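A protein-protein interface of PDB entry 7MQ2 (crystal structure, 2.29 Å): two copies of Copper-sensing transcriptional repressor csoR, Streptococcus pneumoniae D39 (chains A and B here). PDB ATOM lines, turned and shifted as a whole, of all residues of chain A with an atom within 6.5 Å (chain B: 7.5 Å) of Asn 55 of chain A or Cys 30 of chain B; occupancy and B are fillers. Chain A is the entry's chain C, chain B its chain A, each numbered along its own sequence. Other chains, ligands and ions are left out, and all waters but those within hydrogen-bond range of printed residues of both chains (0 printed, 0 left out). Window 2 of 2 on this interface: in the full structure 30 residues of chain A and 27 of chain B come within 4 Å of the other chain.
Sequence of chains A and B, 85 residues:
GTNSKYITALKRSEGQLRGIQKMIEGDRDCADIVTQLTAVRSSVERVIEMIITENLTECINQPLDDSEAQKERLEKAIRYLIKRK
The side-chain amide nitrogen of Asn 55 of chain A lies within hydrogen-bond range of the side-chain sulfur of Cys 30 of chain B, at 2.7 Å.
The side-chain amide oxygen of Asn 55 of chain A lies close to the backbone carbonyl oxygen of Ile 52 of chain A (2.8 Å).
OD2 of Asp 29 of chain B lies within hydrogen-bond range of N of Ala 31 of chain B (3.0 Å).
The backbone carbonyl oxygen of Ala 31 of chain B lies within hydrogen-bond range of the side-chain hydroxyl of Thr 35 of chain B, at 2.8 Å.
Among the printed residues, pairs that only touch across the chains: Ile 51 of chain A with Cys 30 of chain B (3.7 Å), Lys 71 of chain A with Ala 31 of chain B (3.7 Å), Ile 52 of chain A with Val 34 of chain B (3.8 Å), Ile 51 of chain A with Ile 33 of chain B (3.8 Å), Ile 51 of chain A with Val 34 of chain B (3.9 Å) and Ile 51 of chain A with Leu 37 of chain B (3.9 Å).
Asn 55 of chain A touches just one residue of chain B: Cys 30 (2.7 Å).
Cys 59 of chain A touches none of the printed residues of chain B.
Printed residues of chain B within 4 Å of Lys 71 of chain A: Ala 31.
Cys 30 of chain B touches two residues of chain A.
Of the printed residues of chain A, Val 34 of chain B touches Ile 51 (3.9 Å) and Ile 52 (3.8 Å).
Of the printed residues of chain A, Leu 37 of chain B touches Ile 51.
The nearest printed residue of chain A that does not touch Ala 31 of chain B is Asn 55 of chain A (5.4 Å).
Of the 12 printed residues of chain A, 4 touch a printed residue of chain B.
Printed residues of chain A that touch a printed residue of chain B: Ile 51, Ile 52, Asn 55 and Lys 71.
Printed residues of chain B that touch a printed residue of chain A: Cys 30, Ala 31, Ile 33, Val 34 and Leu 37.
Among the printed residues, no Asp or Glu carboxylate lies within 4 Å of a Lys or Arg side-chain nitrogen of the other chain.
No position is printed for both chains.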
ATOM      1  N   MET A  50     -18.151 -12.647  -9.557  1.00  0.00           N
ATOM      2  CA  MET A  50     -18.401 -13.028 -10.947  1.00  0.00           C
ATOM      3  C   MET A  50     -18.626 -14.543 -11.167  1.00  0.00           C
ATOM      4  O   MET A  50     -19.508 -14.906 -11.931  1.00  0.00           O
ATOM      5  CB  MET A  50     -17.238 -12.553 -11.808  1.00  0.00           C
ATOM      6  CG  MET A  50     -17.369 -11.126 -12.350  1.00  0.00           C
ATOM      7  SD  MET A  50     -15.952 -10.725 -13.653  1.00  0.00           S
ATOM      8  CE  MET A  50     -14.396 -11.601 -12.897  1.00  0.00           C
ATOM      9  N   ILE A  51     -17.884 -15.393 -10.439  1.00  0.00           N
ATOM     10  CA  ILE A  51     -18.053 -16.844 -10.552  1.00  0.00           C
ATOM     11  C   ILE A  51     -19.389 -17.300  -9.953  1.00  0.00           C
ATOM     12  O   ILE A  51     -20.121 -18.096 -10.574  1.00  0.00           O
ATOM     13  CB  ILE A  51     -16.836 -17.560  -9.925  1.00  0.00           C
ATOM     14  CG1 ILE A  51     -15.661 -17.517 -10.899  1.00  0.00           C
ATOM     15  CG2 ILE A  51     -17.099 -19.019  -9.592  1.00  0.00           C
ATOM     16  CD1 ILE A  51     -14.349 -17.817 -10.253  1.00  0.00           C
ATOM     17  N   ILE A  52     -19.755 -16.749  -8.782  1.00  0.00           N
ATOM     18  CA  ILE A  52     -21.018 -17.089  -8.113  1.00  0.00           C
ATOM     19  C   ILE A  52     -22.237 -16.629  -8.921  1.00  0.00           C
ATOM     20  O   ILE A  52     -23.193 -17.396  -9.141  1.00  0.00           O
ATOM     21  CB  ILE A  52     -21.009 -16.495  -6.699  1.00  0.00           C
ATOM     22  CG1 ILE A  52     -20.033 -17.272  -5.828  1.00  0.00           C
ATOM     23  CG2 ILE A  52     -22.418 -16.478  -6.068  1.00  0.00           C
ATOM     24  CD1 ILE A  52     -19.871 -16.726  -4.462  1.00  0.00           C
ATOM     25  N   THR A  53     -22.188 -15.418  -9.462  1.00  0.00           N
ATOM     26  CA  THR A  53     -23.323 -14.979 -10.266  1.00  0.00           C
ATOM     27  C   THR A  53     -23.305 -15.523 -11.686  1.00  0.00           C
ATOM     28  O   THR A  53     -24.332 -15.441 -12.372  1.00  0.00           O
ATOM     29  CB  THR A  53     -23.356 -13.466 -10.351  1.00  0.00           C
ATOM     30  OG1 THR A  53     -22.191 -13.047 -11.076  1.00  0.00           O
ATOM     31  CG2 THR A  53     -23.424 -12.839  -8.938  1.00  0.00           C
ATOM     32  N   GLU A  54     -22.156 -16.034 -12.146  1.00  0.00           N
ATOM     33  CA  GLU A  54     -22.121 -16.870 -13.338  1.00  0.00           C
ATOM     34  C   GLU A  54     -22.952 -18.135 -13.160  1.00  0.00           C
ATOM     35  O   GLU A  54     -23.820 -18.413 -13.993  1.00  0.00           O
ATOM     36  CB  GLU A  54     -20.672 -17.199 -13.697  1.00  0.00           C
ATOM     37  CG  GLU A  54     -20.487 -18.468 -14.528  1.00  0.00           C
ATOM     38  CD  GLU A  54     -19.051 -18.818 -14.697  1.00  0.00           C
ATOM     39  OE1 GLU A  54     -18.601 -19.711 -13.949  1.00  0.00           O
ATOM     40  OE2 GLU A  54     -18.394 -18.225 -15.572  1.00  0.00           O
ATOM     41  N   ASN A  55     -22.722 -18.915 -12.081  1.00  0.00           N
ATOM     42  CA  ASN A  55     -23.399 -20.216 -12.112  1.00  0.00           C
ATOM     43  C   ASN A  55     -24.840 -20.152 -11.598  1.00  0.00           C
ATOM     44  O   ASN A  55     -25.694 -20.866 -12.135  1.00  0.00           O
ATOM     45  CB  ASN A  55     -22.671 -21.361 -11.380  1.00  0.00           C
ATOM     46  CG  ASN A  55     -22.523 -21.185  -9.854  1.00  0.00           C
ATOM     47  OD1 ASN A  55     -22.890 -20.224  -9.240  1.00  0.00           O
ATOM     48  ND2 ASN A  55     -22.198 -22.274  -9.237  1.00  0.00           N
ATOM     49  N   LEU A  56     -25.142 -19.274 -10.614  1.00  0.00           N
ATOM     50  CA  LEU A  56     -26.469 -19.273  -9.998  1.00  0.00           C
ATOM     51  C   LEU A  56     -27.574 -18.729 -10.890  1.00  0.00           C
ATOM     52  O   LEU A  56     -28.742 -18.924 -10.560  1.00  0.00           O
ATOM     53  CB  LEU A  56     -26.466 -18.478  -8.695  1.00  0.00           C
ATOM     54  CG  LEU A  56     -25.675 -19.043  -7.519  1.00  0.00           C
ATOM     55  CD1 LEU A  56     -26.151 -18.413  -6.265  1.00  0.00           C
ATOM     56  CD2 LEU A  56     -25.830 -20.565  -7.378  1.00  0.00           C
ATOM     57  N   THR A  57     -27.242 -18.077 -12.003  1.00  0.00           N
ATOM     58  CA  THR A  57     -28.198 -17.919 -13.097  1.00  0.00           C
ATOM     59  C   THR A  57     -28.646 -19.271 -13.666  1.00  0.00           C
ATOM     60  O   THR A  57     -29.849 -19.537 -13.780  1.00  0.00           O
ATOM     61  CB  THR A  57     -27.583 -17.046 -14.196  1.00  0.00           C
ATOM     62  OG1 THR A  57     -27.209 -15.765 -13.658  1.00  0.00           O
ATOM     63  CG2 THR A  57     -28.578 -16.842 -15.342  1.00  0.00           C
ATOM     64  N   GLU A  58     -27.699 -20.152 -14.005  1.00  0.00           N
ATOM     65  CA  GLU A  58     -28.036 -21.441 -14.603  1.00  0.00           C
ATOM     66  C   GLU A  58     -27.863 -22.610 -13.631  1.00  0.00           C
ATOM     67  O   GLU A  58     -27.737 -23.762 -14.062  1.00  0.00           O
ATOM     68  CB  GLU A  58     -27.220 -21.681 -15.879  1.00  0.00           C
ATOM     69  CG  GLU A  58     -25.699 -21.735 -15.721  1.00  0.00           C
ATOM     70  CD  GLU A  58     -25.005 -20.482 -16.218  1.00  0.00           C
ATOM     71  OE1 GLU A  58     -25.648 -19.409 -16.267  1.00  0.00           O
ATOM     72  OE2 GLU A  58     -23.819 -20.582 -16.597  1.00  0.00           O
ATOM     73  N   CYS A  59     -27.874 -22.343 -12.327  1.00  0.00           N
ATOM     74  CA  CYS A  59     -27.982 -23.418 -11.348  1.00  0.00           C
ATOM     75  C   CYS A  59     -29.417 -23.472 -10.824  1.00  0.00           C
ATOM     76  O   CYS A  59     -30.368 -23.187 -11.559  1.00  0.00           O
ATOM     77  CB  CYS A  59     -26.981 -23.216 -10.200  1.00  0.00           C
ATOM     78  SG  CYS A  59     -26.663 -24.647  -9.125  1.00  0.00           S
ATOM     79  N   ALA A  69     -26.487 -30.473  -8.092  1.00  0.00           N
ATOM     80  CA  ALA A  69     -26.850 -29.075  -7.952  1.00  0.00           C
ATOM     81  C   ALA A  69     -25.781 -28.305  -7.143  1.00  0.00           C
ATOM     82  O   ALA A  69     -24.805 -27.800  -7.719  1.00  0.00           O
ATOM     83  CB  ALA A  69     -28.228 -28.958  -7.310  1.00  0.00           C
ATOM     84  N   LYS A  71     -24.058 -25.426  -5.270  1.00  0.00           N
ATOM     85  CA  LYS A  71     -22.862 -24.716  -4.839  1.00  0.00           C
ATOM     86  C   LYS A  71     -23.234 -23.556  -3.919  1.00  0.00           C
ATOM     87  O   LYS A  71     -24.049 -22.703  -4.292  1.00  0.00           O
ATOM     88  CB  LYS A  71     -22.102 -24.195  -6.060  1.00  0.00           C
ATOM     89  N   ASP B  27     -11.321 -26.991 -15.290  1.00  0.00           N
ATOM     90  CA  ASP B  27     -12.795 -26.928 -15.195  1.00  0.00           C
ATOM     91  C   ASP B  27     -13.313 -27.553 -13.902  1.00  0.00           C
ATOM     92  O   ASP B  27     -14.351 -28.228 -13.874  1.00  0.00           O
ATOM     93  CB  ASP B  27     -13.475 -27.552 -16.403  1.00  0.00           C
ATOM     94  CG  ASP B  27     -13.574 -26.597 -17.533  1.00  0.00           C
ATOM     95  OD1 ASP B  27     -13.173 -26.959 -18.645  1.00  0.00           O
ATOM     96  OD2 ASP B  27     -14.041 -25.459 -17.313  1.00  0.00           O
ATOM     97  N   ARG B  28     -12.573 -27.302 -12.823  1.00  0.00           N
ATOM     98  CA  ARG B  28     -12.987 -27.666 -11.492  1.00  0.00           C
ATOM     99  C   ARG B  28     -14.260 -26.899 -11.092  1.00  0.00           C
ATOM    100  O   ARG B  28     -14.673 -25.916 -11.727  1.00  0.00           O
ATOM    101  CB  ARG B  28     -11.846 -27.411 -10.494  1.00  0.00           C
ATOM    102  CG  ARG B  28     -10.666 -28.289 -10.668  1.00  0.00           C
ATOM    103  CD  ARG B  28     -10.981 -29.746 -10.187  1.00  0.00           C
ATOM    104  NE  ARG B  28     -11.247 -29.725  -8.747  1.00  0.00           N
ATOM    105  CZ  ARG B  28     -10.309 -29.696  -7.800  1.00  0.00           C
ATOM    106  NH1 ARG B  28      -9.003 -29.758  -8.109  1.00  0.00           N
ATOM    107  NH2 ARG B  28     -10.681 -29.620  -6.525  1.00  0.00           N
ATOM    108  N   ASP B  29     -14.933 -27.446 -10.088  1.00  0.00           N
ATOM    109  CA  ASP B  29     -16.256 -27.000  -9.691  1.00  0.00           C
ATOM    110  C   ASP B  29     -16.157 -25.602  -9.078  1.00  0.00           C
ATOM    111  O   ASP B  29     -15.196 -25.299  -8.369  1.00  0.00           O
ATOM    112  CB  ASP B  29     -16.810 -28.011  -8.677  1.00  0.00           C
ATOM    113  CG  ASP B  29     -18.212 -27.757  -8.315  1.00  0.00           C
ATOM    114  OD1 ASP B  29     -19.113 -28.355  -8.952  1.00  0.00           O
ATOM    115  OD2 ASP B  29     -18.424 -26.945  -7.395  1.00  0.00           O
ATOM    116  N   CYS B  30     -17.151 -24.757  -9.370  1.00  0.00           N
ATOM    117  CA  CYS B  30     -17.111 -23.347  -8.974  1.00  0.00           C
ATOM    118  C   CYS B  30     -17.173 -23.149  -7.466  1.00  0.00           C
ATOM    119  O   CYS B  30     -16.530 -22.233  -6.967  1.00  0.00           O
ATOM    120  CB  CYS B  30     -18.236 -22.581  -9.646  1.00  0.00           C
ATOM    121  SG  CYS B  30     -19.741 -23.380  -9.466  1.00  0.00           S
ATOM    122  N   ALA B  31     -17.785 -24.083  -6.720  1.00  0.00           N
ATOM    123  CA  ALA B  31     -17.732 -24.034  -5.257  1.00  0.00           C
ATOM    124  C   ALA B  31     -16.342 -24.331  -4.711  1.00  0.00           C
ATOM    125  O   ALA B  31     -15.907 -23.678  -3.748  1.00  0.00           O
ATOM    126  CB  ALA B  31     -18.733 -25.013  -4.658  1.00  0.00           C
ATOM    127  N   ASP B  32     -15.627 -25.298  -5.324  1.00  0.00           N
ATOM    128  CA  ASP B  32     -14.220 -25.536  -4.994  1.00  0.00           C
ATOM    129  C   ASP B  32     -13.329 -24.337  -5.333  1.00  0.00           C
ATOM    130  O   ASP B  32     -12.391 -24.030  -4.571  1.00  0.00           O
ATOM    131  CB  ASP B  32     -13.717 -26.761  -5.754  1.00  0.00           C
ATOM    132  CG  ASP B  32     -14.267 -28.067  -5.201  1.00  0.00           C
ATOM    133  OD1 ASP B  32     -15.181 -28.040  -4.333  1.00  0.00           O
ATOM    134  OD2 ASP B  32     -13.801 -29.123  -5.682  1.00  0.00           O
ATOM    135  N   ILE B  33     -13.599 -23.679  -6.480  1.00  0.00           N
ATOM    136  CA  ILE B  33     -12.901 -22.447  -6.862  1.00  0.00           C
ATOM    137  C   ILE B  33     -13.110 -21.369  -5.809  1.00  0.00           C
ATOM    138  O   ILE B  33     -12.129 -20.860  -5.253  1.00  0.00           O
ATOM    139  CB  ILE B  33     -13.364 -21.917  -8.238  1.00  0.00           C
ATOM    140  CG1 ILE B  33     -13.294 -22.931  -9.386  1.00  0.00           C
ATOM    141  CG2 ILE B  33     -12.523 -20.715  -8.617  1.00  0.00           C
ATOM    142  CD1 ILE B  33     -12.018 -23.372  -9.826  1.00  0.00           C
ATOM    143  N   VAL B  34     -14.394 -21.137  -5.417  1.00  0.00           N
ATOM    144  CA  VAL B  34     -14.794 -20.052  -4.499  1.00  0.00           C
ATOM    145  C   VAL B  34     -14.214 -20.283  -3.112  1.00  0.00           C
ATOM    146  O   VAL B  34     -13.637 -19.358  -2.520  1.00  0.00           O
ATOM    147  CB  VAL B  34     -16.331 -19.904  -4.465  1.00  0.00           C
ATOM    148  CG1 VAL B  34     -16.817 -19.091  -3.237  1.00  0.00           C
ATOM    149  CG2 VAL B  34     -16.828 -19.227  -5.718  1.00  0.00           C
ATOM    150  N   THR B  35     -14.211 -21.546  -2.661  1.00  0.00           N
ATOM    151  CA  THR B  35     -13.576 -21.962  -1.398  1.00  0.00           C
ATOM    152  C   THR B  35     -12.071 -21.657  -1.346  1.00  0.00           C
ATOM    153  O   THR B  35     -11.577 -21.083  -0.358  1.00  0.00           O
ATOM    154  CB  THR B  35     -13.833 -23.476  -1.208  1.00  0.00           C
ATOM    155  OG1 THR B  35     -15.237 -23.706  -1.005  1.00  0.00           O
ATOM    156  CG2 THR B  35     -13.058 -24.043  -0.050  1.00  0.00           C
ATOM    157  N   GLN B  36     -11.345 -21.928  -2.442  1.00  0.00           N
ATOM    158  CA  GLN B  36      -9.917 -21.572  -2.452  1.00  0.00           C
ATOM    159  C   GLN B  36      -9.664 -20.050  -2.592  1.00  0.00           C
ATOM    160  O   GLN B  36      -8.752 -19.508  -1.953  1.00  0.00           O
ATOM    161  CB  GLN B  36      -9.237 -22.376  -3.554  1.00  0.00           C
ATOM    162  CG  GLN B  36      -9.292 -23.898  -3.323  1.00  0.00           C
ATOM    163  CD  GLN B  36      -8.241 -24.387  -2.335  1.00  0.00           C
ATOM    164  OE1 GLN B  36      -7.188 -24.876  -2.737  1.00  0.00           O
ATOM    165  NE2 GLN B  36      -8.553 -24.328  -1.042  1.00  0.00           N
ATOM    166  N   LEU B  37     -10.485 -19.359  -3.386  1.00  0.00           N
ATOM    167  CA  LEU B  37     -10.424 -17.897  -3.517  1.00  0.00           C
ATOM    168  C   LEU B  37     -10.717 -17.185  -2.193  1.00  0.00           C
ATOM    169  O   LEU B  37     -10.026 -16.224  -1.827  1.00  0.00           O
ATOM    170  CB  LEU B  37     -11.423 -17.467  -4.584  1.00  0.00           C
ATOM    171  CG  LEU B  37     -11.024 -17.669  -6.052  1.00  0.00           C
ATOM    172  CD1 LEU B  37     -12.128 -17.358  -7.062  1.00  0.00           C
ATOM    173  CD2 LEU B  37      -9.831 -16.789  -6.292  1.00  0.00           C
